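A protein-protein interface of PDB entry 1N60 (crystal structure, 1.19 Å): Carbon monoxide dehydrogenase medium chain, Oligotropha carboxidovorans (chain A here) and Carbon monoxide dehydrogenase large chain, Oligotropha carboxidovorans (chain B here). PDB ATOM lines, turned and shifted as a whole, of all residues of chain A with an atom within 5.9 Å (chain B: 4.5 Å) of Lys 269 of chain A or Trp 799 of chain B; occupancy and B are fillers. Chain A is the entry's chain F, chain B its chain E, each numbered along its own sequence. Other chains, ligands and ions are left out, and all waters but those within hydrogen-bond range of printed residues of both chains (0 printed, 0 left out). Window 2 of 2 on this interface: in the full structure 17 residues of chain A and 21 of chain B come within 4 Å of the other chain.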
ATOM      1  N   VAL A 247     -40.044 -16.512  -2.253  1.00  0.00           N
ATOM      2  CA  VAL A 247     -38.982 -15.573  -2.605  1.00  0.00           C
ATOM      3  C   VAL A 247     -39.434 -14.676  -3.695  1.00  0.00           C
ATOM      4  O   VAL A 247     -39.248 -13.479  -3.629  1.00  0.00           O
ATOM      5  CB  VAL A 247     -37.701 -16.291  -2.981  1.00  0.00           C
ATOM      6  CG1 VAL A 247     -36.684 -15.352  -3.631  1.00  0.00           C
ATOM      7  CG2 VAL A 247     -37.087 -16.915  -1.726  1.00  0.00           C
ATOM      8  N   GLU A 251     -39.633 -10.703  -3.097  1.00  0.00           N
ATOM      9  CA  GLU A 251     -38.827  -9.805  -3.896  1.00  0.00           C
ATOM     10  C   GLU A 251     -39.672  -8.797  -4.633  1.00  0.00           C
ATOM     11  O   GLU A 251     -39.337  -7.646  -4.778  1.00  0.00           O
ATOM     12  CB  GLU A 251     -38.011 -10.608  -4.896  1.00  0.00           C
ATOM     13  CG  GLU A 251     -36.847 -11.373  -4.285  1.00  0.00           C
ATOM     14  CD  GLU A 251     -36.168 -12.247  -5.284  1.00  0.00           C
ATOM     15  OE1 GLU A 251     -36.663 -12.439  -6.432  1.00  0.00           O
ATOM     16  OE2 GLU A 251     -35.072 -12.742  -4.932  1.00  0.00           O
ATOM     17  N   PRO A 263     -26.628  -1.709  -4.353  1.00  0.00           N
ATOM     18  CA  PRO A 263     -27.707  -1.211  -5.209  1.00  0.00           C
ATOM     19  C   PRO A 263     -28.969  -1.955  -4.977  1.00  0.00           C
ATOM     20  O   PRO A 263     -28.974  -3.074  -4.436  1.00  0.00           O
ATOM     21  CB  PRO A 263     -27.194  -1.481  -6.605  1.00  0.00           C
ATOM     22  CG  PRO A 263     -26.332  -2.711  -6.431  1.00  0.00           C
ATOM     23  CD  PRO A 263     -25.670  -2.555  -5.072  1.00  0.00           C
ATOM     24  N   ALA A 264     -30.067  -1.344  -5.394  1.00  0.00           N
ATOM     25  CA  ALA A 264     -31.381  -1.932  -5.162  1.00  0.00           C
ATOM     26  C   ALA A 264     -31.543  -3.368  -5.594  1.00  0.00           C
ATOM     27  O   ALA A 264     -32.117  -4.196  -4.890  1.00  0.00           O
ATOM     28  CB  ALA A 264     -32.426  -1.067  -5.825  1.00  0.00           C
ATOM     29  N   GLU A 265     -30.982  -3.700  -6.743  1.00  0.00           N
ATOM     30  CA  GLU A 265     -31.123  -5.044  -7.250  1.00  0.00           C
ATOM     31  C   GLU A 265     -30.501  -6.099  -6.331  1.00  0.00           C
ATOM     32  O   GLU A 265     -31.004  -7.200  -6.151  1.00  0.00           O
ATOM     33  CB  GLU A 265     -30.616  -5.113  -8.685  1.00  0.00           C
ATOM     34  CG  GLU A 265     -29.162  -4.739  -8.936  1.00  0.00           C
ATOM     35  CD  GLU A 265     -28.850  -3.250  -9.102  1.00  0.00           C
ATOM     36  OE1 GLU A 265     -29.734  -2.368  -8.834  1.00  0.00           O
ATOM     37  OE2 GLU A 265     -27.677  -2.955  -9.524  1.00  0.00           O
ATOM     38  N   TYR A 266     -29.364  -5.748  -5.738  1.00  0.00           N
ATOM     39  CA  TYR A 266     -28.711  -6.650  -4.813  1.00  0.00           C
ATOM     40  C   TYR A 266     -29.580  -6.820  -3.589  1.00  0.00           C
ATOM     41  O   TYR A 266     -29.773  -7.921  -3.069  1.00  0.00           O
ATOM     42  CB  TYR A 266     -27.347  -6.047  -4.385  1.00  0.00           C
ATOM     43  CG  TYR A 266     -26.683  -6.736  -3.255  1.00  0.00           C
ATOM     44  CD1 TYR A 266     -26.380  -8.056  -3.352  1.00  0.00           C
ATOM     45  CD2 TYR A 266     -26.349  -6.074  -2.062  1.00  0.00           C
ATOM     46  CE1 TYR A 266     -25.702  -8.726  -2.339  1.00  0.00           C
ATOM     47  CE2 TYR A 266     -25.716  -6.762  -1.066  1.00  0.00           C
ATOM     48  CZ  TYR A 266     -25.385  -8.072  -1.179  1.00  0.00           C
ATOM     49  OH  TYR A 266     -24.732  -8.701  -0.141  1.00  0.00           O
ATOM     50  N   ARG A 267     -30.046  -5.698  -3.079  1.00  0.00           N
ATOM     51  CA  ARG A 267     -30.807  -5.748  -1.859  1.00  0.00           C
ATOM     52  C   ARG A 267     -32.133  -6.513  -2.011  1.00  0.00           C
ATOM     53  O   ARG A 267     -32.557  -7.230  -1.101  1.00  0.00           O
ATOM     54  CB  ARG A 267     -31.034  -4.335  -1.371  1.00  0.00           C
ATOM     55  CG  ARG A 267     -29.687  -3.678  -1.012  1.00  0.00           C
ATOM     56  CD  ARG A 267     -29.874  -2.280  -0.488  1.00  0.00           C
ATOM     57  NE  ARG A 267     -30.342  -2.298   0.861  1.00  0.00           N
ATOM     58  CZ  ARG A 267     -30.414  -1.198   1.557  1.00  0.00           C
ATOM     59  NH1 ARG A 267     -30.220  -0.026   0.998  1.00  0.00           N
ATOM     60  NH2 ARG A 267     -30.701  -1.263   2.834  1.00  0.00           N
ATOM     61  N   THR A 268     -32.728  -6.425  -3.185  1.00  0.00           N
ATOM     62  CA  THR A 268     -33.915  -7.237  -3.487  1.00  0.00           C
ATOM     63  C   THR A 268     -33.588  -8.717  -3.415  1.00  0.00           C
ATOM     64  O   THR A 268     -34.278  -9.518  -2.764  1.00  0.00           O
ATOM     65  CB  THR A 268     -34.486  -6.825  -4.836  1.00  0.00           C
ATOM     66  OG1 THR A 268     -35.123  -5.548  -4.664  1.00  0.00           O
ATOM     67  CG2 THR A 268     -35.518  -7.813  -5.360  1.00  0.00           C
ATOM     68  N   LYS A 269     -32.477  -9.100  -4.056  1.00  0.00           N
ATOM     69  CA  LYS A 269     -32.089 -10.473  -3.993  1.00  0.00           C
ATOM     70  C   LYS A 269     -31.750 -10.905  -2.577  1.00  0.00           C
ATOM     71  O   LYS A 269     -32.062 -12.034  -2.160  1.00  0.00           O
ATOM     72  CB  LYS A 269     -30.906 -10.790  -4.953  1.00  0.00           C
ATOM     73  CG  LYS A 269     -31.288 -10.657  -6.395  1.00  0.00           C
ATOM     74  CD  LYS A 269     -32.511 -11.466  -6.882  1.00  0.00           C
ATOM     75  CE  LYS A 269     -32.326 -12.938  -6.692  1.00  0.00           C
ATOM     76  NZ  LYS A 269     -33.600 -13.641  -7.063  1.00  0.00           N
ATOM     77  N   MET A 270     -31.152 -10.002  -1.806  1.00  0.00           N
ATOM     78  CA  MET A 270     -30.806 -10.350  -0.442  1.00  0.00           C
ATOM     79  C   MET A 270     -32.028 -10.467   0.434  1.00  0.00           C
ATOM     80  O   MET A 270     -32.025 -11.302   1.342  1.00  0.00           O
ATOM     81  CB  MET A 270     -29.823  -9.361   0.168  1.00  0.00           C
ATOM     82  CG  MET A 270     -28.452  -9.404  -0.497  1.00  0.00           C
ATOM     83  SD  MET A 270     -27.700 -11.032  -0.559  1.00  0.00           S
ATOM     84  CE  MET A 270     -28.130 -11.574  -2.254  1.00  0.00           C
ATOM     85  N   ALA A 271     -33.096  -9.697   0.141  1.00  0.00           N
ATOM     86  CA  ALA A 271     -34.339  -9.960   0.845  1.00  0.00           C
ATOM     87  C   ALA A 271     -34.736 -11.421   0.670  1.00  0.00           C
ATOM     88  O   ALA A 271     -35.234 -12.080   1.589  1.00  0.00           O
ATOM     89  CB  ALA A 271     -35.401  -9.055   0.360  1.00  0.00           C
ATOM     90  N   GLY A 272     -34.634 -11.878  -0.575  1.00  0.00           N
ATOM     91  CA  GLY A 272     -34.974 -13.243  -0.897  1.00  0.00           C
ATOM     92  C   GLY A 272     -34.097 -14.270  -0.202  1.00  0.00           C
ATOM     93  O   GLY A 272     -34.585 -15.266   0.329  1.00  0.00           O
ATOM     94  N   VAL A 273     -32.786 -13.993  -0.175  1.00  0.00           N
ATOM     95  CA  VAL A 273     -31.904 -14.926   0.462  1.00  0.00           C
ATOM     96  C   VAL A 273     -32.146 -14.958   1.959  1.00  0.00           C
ATOM     97  O   VAL A 273     -32.165 -15.997   2.575  1.00  0.00           O
ATOM     98  CB  VAL A 273     -30.425 -14.625   0.124  1.00  0.00           C
ATOM     99  CG1 VAL A 273     -29.498 -15.601   0.906  1.00  0.00           C
ATOM    100  CG2 VAL A 273     -30.180 -14.761  -1.341  1.00  0.00           C
ATOM    101  N   MET A 274     -32.291 -13.802   2.570  1.00  0.00           N
ATOM    102  CA  MET A 274     -32.566 -13.777   3.990  1.00  0.00           C
ATOM    103  C   MET A 274     -33.865 -14.522   4.270  1.00  0.00           C
ATOM    104  O   MET A 274     -33.985 -15.233   5.266  1.00  0.00           O
ATOM    105  CB  MET A 274     -32.616 -12.336   4.467  1.00  0.00           C
ATOM    106  CG  MET A 274     -31.263 -11.641   4.453  1.00  0.00           C
ATOM    107  SD  MET A 274     -29.943 -12.465   5.346  1.00  0.00           S
ATOM    108  CE  MET A 274     -29.125 -13.222   4.107  1.00  0.00           C
ATOM    109  N   ASP B 671     -23.539 -16.502  -2.995  1.00  0.00           N
ATOM    110  CA  ASP B 671     -24.920 -16.071  -3.112  1.00  0.00           C
ATOM    111  C   ASP B 671     -25.190 -14.749  -2.424  1.00  0.00           C
ATOM    112  O   ASP B 671     -26.095 -14.015  -2.852  1.00  0.00           O
ATOM    113  CB  ASP B 671     -25.850 -17.156  -2.619  1.00  0.00           C
ATOM    114  CG  ASP B 671     -25.836 -18.324  -3.531  1.00  0.00           C
ATOM    115  OD1 ASP B 671     -25.759 -18.148  -4.788  1.00  0.00           O
ATOM    116  OD2 ASP B 671     -25.888 -19.475  -3.068  1.00  0.00           O
ATOM    117  N   THR B 672     -24.421 -14.427  -1.407  1.00  0.00           N
ATOM    118  CA  THR B 672     -24.547 -13.137  -0.750  1.00  0.00           C
ATOM    119  C   THR B 672     -23.371 -12.237  -0.976  1.00  0.00           C
ATOM    120  O   THR B 672     -23.466 -11.064  -0.730  1.00  0.00           O
ATOM    121  CB  THR B 672     -24.701 -13.317   0.760  1.00  0.00           C
ATOM    122  OG1 THR B 672     -23.544 -14.013   1.231  1.00  0.00           O
ATOM    123  CG2 THR B 672     -25.953 -14.090   1.076  1.00  0.00           C
ATOM    124  N   GLY B 673     -22.245 -12.800  -1.409  1.00  0.00           N
ATOM    125  CA  GLY B 673     -21.013 -12.049  -1.484  1.00  0.00           C
ATOM    126  C   GLY B 673     -20.255 -11.939  -0.197  1.00  0.00           C
ATOM    127  O   GLY B 673     -19.223 -11.295  -0.183  1.00  0.00           O
ATOM    128  N   ALA B 795     -19.678  -7.205   0.360  1.00  0.00           N
ATOM    129  CA  ALA B 795     -20.640  -8.180  -0.088  1.00  0.00           C
ATOM    130  C   ALA B 795     -21.373  -7.819  -1.348  1.00  0.00           C
ATOM    131  O   ALA B 795     -21.485  -8.667  -2.224  1.00  0.00           O
ATOM    132  CB  ALA B 795     -21.584  -8.530   1.060  1.00  0.00           C
ATOM    133  N   TRP B 796     -21.767  -6.578  -1.529  1.00  0.00           N
ATOM    134  CA  TRP B 796     -22.515  -6.288  -2.713  1.00  0.00           C
ATOM    135  C   TRP B 796     -21.597  -6.414  -3.948  1.00  0.00           C
ATOM    136  O   TRP B 796     -22.042  -6.865  -4.995  1.00  0.00           O
ATOM    137  CB  TRP B 796     -23.181  -4.914  -2.694  1.00  0.00           C
ATOM    138  CG  TRP B 796     -22.400  -3.686  -2.843  1.00  0.00           C
ATOM    139  CD1 TRP B 796     -21.942  -2.894  -1.852  1.00  0.00           C
ATOM    140  CD2 TRP B 796     -22.035  -3.077  -4.057  1.00  0.00           C
ATOM    141  NE1 TRP B 796     -21.325  -1.793  -2.385  1.00  0.00           N
ATOM    142  CE2 TRP B 796     -21.356  -1.877  -3.734  1.00  0.00           C
ATOM    143  CE3 TRP B 796     -22.244  -3.381  -5.419  1.00  0.00           C
ATOM    144  CZ2 TRP B 796     -20.850  -0.998  -4.685  1.00  0.00           C
ATOM    145  CZ3 TRP B 796     -21.742  -2.490  -6.364  1.00  0.00           C
ATOM    146  CH2 TRP B 796     -21.048  -1.315  -5.970  1.00  0.00           C
ATOM    147  N   ARG B 797     -20.345  -5.994  -3.801  1.00  0.00           N
ATOM    148  CA  ARG B 797     -19.452  -6.094  -4.922  1.00  0.00           C
ATOM    149  C   ARG B 797     -19.080  -7.503  -5.230  1.00  0.00           C
ATOM    150  O   ARG B 797     -19.015  -7.851  -6.417  1.00  0.00           O
ATOM    151  CB  ARG B 797     -18.214  -5.245  -4.690  1.00  0.00           C
ATOM    152  CG  ARG B 797     -18.504  -3.837  -5.181  1.00  0.00           C
ATOM    153  CD  ARG B 797     -17.494  -2.807  -4.770  1.00  0.00           C
ATOM    154  NE  ARG B 797     -17.819  -2.315  -3.446  1.00  0.00           N
ATOM    155  CZ  ARG B 797     -17.782  -1.080  -3.037  1.00  0.00           C
ATOM    156  NH1 ARG B 797     -17.368  -0.096  -3.815  1.00  0.00           N
ATOM    157  NH2 ARG B 797     -18.128  -0.851  -1.794  1.00  0.00           N
ATOM    158  N   LEU B 798     -18.927  -8.387  -4.254  1.00  0.00           N
ATOM    159  CA  LEU B 798     -18.638  -9.766  -4.583  1.00  0.00           C
ATOM    160  C   LEU B 798     -19.915 -10.458  -5.073  1.00  0.00           C
ATOM    161  O   LEU B 798     -19.848 -11.340  -5.919  1.00  0.00           O
ATOM    162  CB  LEU B 798     -18.071 -10.549  -3.420  1.00  0.00           C
ATOM    163  CG  LEU B 798     -16.724  -9.974  -2.942  1.00  0.00           C
ATOM    164  CD1 LEU B 798     -16.134 -10.927  -1.957  1.00  0.00           C
ATOM    165  CD2 LEU B 798     -15.800  -9.762  -4.108  1.00  0.00           C
ATOM    166  N   TRP B 799     -21.085 -10.031  -4.608  1.00  0.00           N
ATOM    167  CA  TRP B 799     -22.325 -10.544  -5.198  1.00  0.00           C
ATOM    168  C   TRP B 799     -22.334 -10.177  -6.688  1.00  0.00           C
ATOM    169  O   TRP B 799     -22.722 -11.017  -7.506  1.00  0.00           O
ATOM    170  CB  TRP B 799     -23.538  -9.921  -4.484  1.00  0.00           C
ATOM    171  CG  TRP B 799     -24.815 -10.381  -5.120  1.00  0.00           C
ATOM    172  CD1 TRP B 799     -25.504 -11.514  -4.794  1.00  0.00           C
ATOM    173  CD2 TRP B 799     -25.561  -9.737  -6.131  1.00  0.00           C
ATOM    174  NE1 TRP B 799     -26.636 -11.612  -5.577  1.00  0.00           N
ATOM    175  CE2 TRP B 799     -26.695 -10.532  -6.394  1.00  0.00           C
ATOM    176  CE3 TRP B 799     -25.412  -8.580  -6.837  1.00  0.00           C
ATOM    177  CZ2 TRP B 799     -27.640 -10.194  -7.312  1.00  0.00           C
ATOM    178  CZ3 TRP B 799     -26.391  -8.231  -7.764  1.00  0.00           C
ATOM    179  CH2 TRP B 799     -27.486  -9.045  -7.994  1.00  0.00           C
ATOM    180  N   LYS B 800     -21.999  -8.944  -7.047  1.00  0.00           N
ATOM    181  CA  LYS B 800     -21.990  -8.532  -8.427  1.00  0.00           C
ATOM    182  C   LYS B 800     -21.027  -9.379  -9.251  1.00  0.00           C
ATOM    183  O   LYS B 800     -21.339  -9.746 -10.363  1.00  0.00           O
ATOM    184  CB  LYS B 800     -21.631  -7.075  -8.579  1.00  0.00           C
ATOM    185  CG  LYS B 800     -22.649  -6.083  -8.188  1.00  0.00           C
ATOM    186  CD  LYS B 800     -23.699  -5.921  -9.204  1.00  0.00           C
ATOM    187  CE  LYS B 800     -24.679  -4.862  -8.771  1.00  0.00           C
ATOM    188  NZ  LYS B 800     -25.571  -4.441  -9.868  1.00  0.00           N
ATOM    189  N   VAL B 801     -19.869  -9.749  -8.689  1.00  0.00           N
ATOM    190  CA  VAL B 801     -18.928 -10.600  -9.391  1.00  0.00           C
ATOM    191  C   VAL B 801     -19.649 -11.873  -9.742  1.00  0.00           C
ATOM    192  O   VAL B 801     -19.612 -12.344 -10.901  1.00  0.00           O
ATOM    193  CB  VAL B 801     -17.689 -10.861  -8.543  1.00  0.00           C
ATOM    194  CG1 VAL B 801     -16.863 -12.004  -9.164  1.00  0.00           C
ATOM    195  CG2 VAL B 801     -16.829  -9.595  -8.403  1.00  0.00           C
ATOM    196  N   GLY B 802     -20.270 -12.508  -8.761  1.00  0.00           N
ATOM    197  CA  GLY B 802     -20.924 -13.769  -9.023  1.00  0.00           C
ATOM    198  C   GLY B 802     -22.139 -13.649  -9.932  1.00  0.00           C
ATOM    199  O   GLY B 802     -22.401 -14.497 -10.771  1.00  0.00           O
ATOM    200  N   GLU B 803     -22.862 -12.565  -9.819  1.00  0.00           N
ATOM    201  CA  GLU B 803     -24.019 -12.320 -10.636  1.00  0.00           C
ATOM    202  C   GLU B 803     -23.575 -12.290 -12.087  1.00  0.00           C
ATOM    203  O   GLU B 803     -24.202 -12.925 -12.921  1.00  0.00           O
ATOM    204  CB  GLU B 803     -24.643 -10.952 -10.220  1.00  0.00           C
ATOM    205  CG  GLU B 803     -25.871 -10.580 -11.035  1.00  0.00           C
ATOM    206  CD  GLU B 803     -27.032 -11.535 -10.906  1.00  0.00           C
ATOM    207  OE1 GLU B 803     -27.175 -12.241  -9.889  1.00  0.00           O
ATOM    208  OE2 GLU B 803     -27.888 -11.615 -11.851  1.00  0.00           O
ATOM    209  N   HIS B 808     -25.909 -17.098 -10.022  1.00  0.00           N
ATOM    210  CA  HIS B 808     -27.142 -16.992  -9.259  1.00  0.00           C
ATOM    211  C   HIS B 808     -28.362 -17.555  -9.962  1.00  0.00           C
ATOM    212  O   HIS B 808     -29.459 -17.333  -9.527  1.00  0.00           O
ATOM    213  CB  HIS B 808     -27.358 -15.556  -8.906  1.00  0.00           C
ATOM    214  CG  HIS B 808     -26.268 -15.013  -8.052  1.00  0.00           C
ATOM    215  ND1 HIS B 808     -25.856 -13.718  -8.147  1.00  0.00           N
ATOM    216  CD2 HIS B 808     -25.485 -15.603  -7.121  1.00  0.00           C
ATOM    217  CE1 HIS B 808     -24.851 -13.522  -7.319  1.00  0.00           C
ATOM    218  NE2 HIS B 808     -24.622 -14.643  -6.672  1.00  0.00           N
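The indole nitrogen of Trp 799 of chain B sits close to a ring nitrogen (ND1) of His 808 of chain B, at 3.4 Å. The side-chain carboxylate (OE2) of Glu 251 of chain A lies within salt-bridge range of the side-chain amino group (NZ) of Lys 269 of chain A, at 2.7 Å. The side-chain sulfur (SD) of Met 270 of chain A lies close to the side-chain hydroxyl (OH) of Tyr 266 of chain A, 3.8 Å away.
Printed residues of chain A that touch a printed residue of chain B: Pro 263, Glu 265, Tyr 266, Lys 269, Met 270 and Val 273. Of the 13 printed residues of chain B, 6 touch a printed residue of chain A. Printed residues of chain B that touch a printed residue of chain A: Asp 671, Thr 672, Ala 795, Trp 796, Trp 799 and Lys 800. Among the printed residues, 12 pairs touch across the chains. Among the printed residues, Asp or Glu carboxylates within 4 Å of a Lys or Arg side-chain nitrogen of the other chain: Glu 265 of chain A with Lys 800 of chain B (2.6 Å).
Of the printed residues of chain B, Pro 263 of chain A touches Trp 796 and Lys 800. Of the printed residues of chain B, Glu 265 of chain A touches Lys 800. Of the printed residues of chain B, Tyr 266 of chain A touches Thr 672, Ala 795, Trp 796 and Trp 799. Of chain B, only Trp 799 comes within 4 Å of Lys 269 of chain A. Of the printed residues of chain B, Met 270 of chain A touches Asp 671, Thr 672 and Trp 799. Of the printed residues of chain A, Asp 671 of chain B touches Met 270. Of chain A, only Tyr 266, Lys 269 and Met 270 come within 4 Å of Trp 799 of chain B. The nearest printed residue of chain B that does not touch Lys 269 of chain A is Glu 803 of chain B (5.6 Å). The nearest printed residue of chain A that does not touch Trp 796 of chain B is Glu 265 of chain A (6.7 Å).
The side-chain amino group (NZ) of Lys 800 of chain B lies within salt-bridge range of the side-chain carboxylate (OE2) of Glu 265 of chain A, 2.6 Å away. OH of Tyr 266 of chain A lies within hydrogen-bond range of O of Thr 672 of chain B (2.7 Å).
Among the printed residues, pairs that only touch across the chains: Pro 263 of chain A with Trp 796 of chain B, Pro 263 of chain A with Lys 800 of chain B, Tyr 266 of chain A with Ala 795 of chain B, Tyr 266 of chain A with Trp 796 of chain B, Tyr 266 of chain A with Trp 799 of chain B, Lys 269 of chain A with Trp 799 of chain B, Met 270 of chain A with Asp 671 of chain B, Met 270 of chain A with Thr 672 of chain B, Met 270 of chain A with Trp 799 of chain B and Val 273 of chain A with Thr 672 of chain B.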
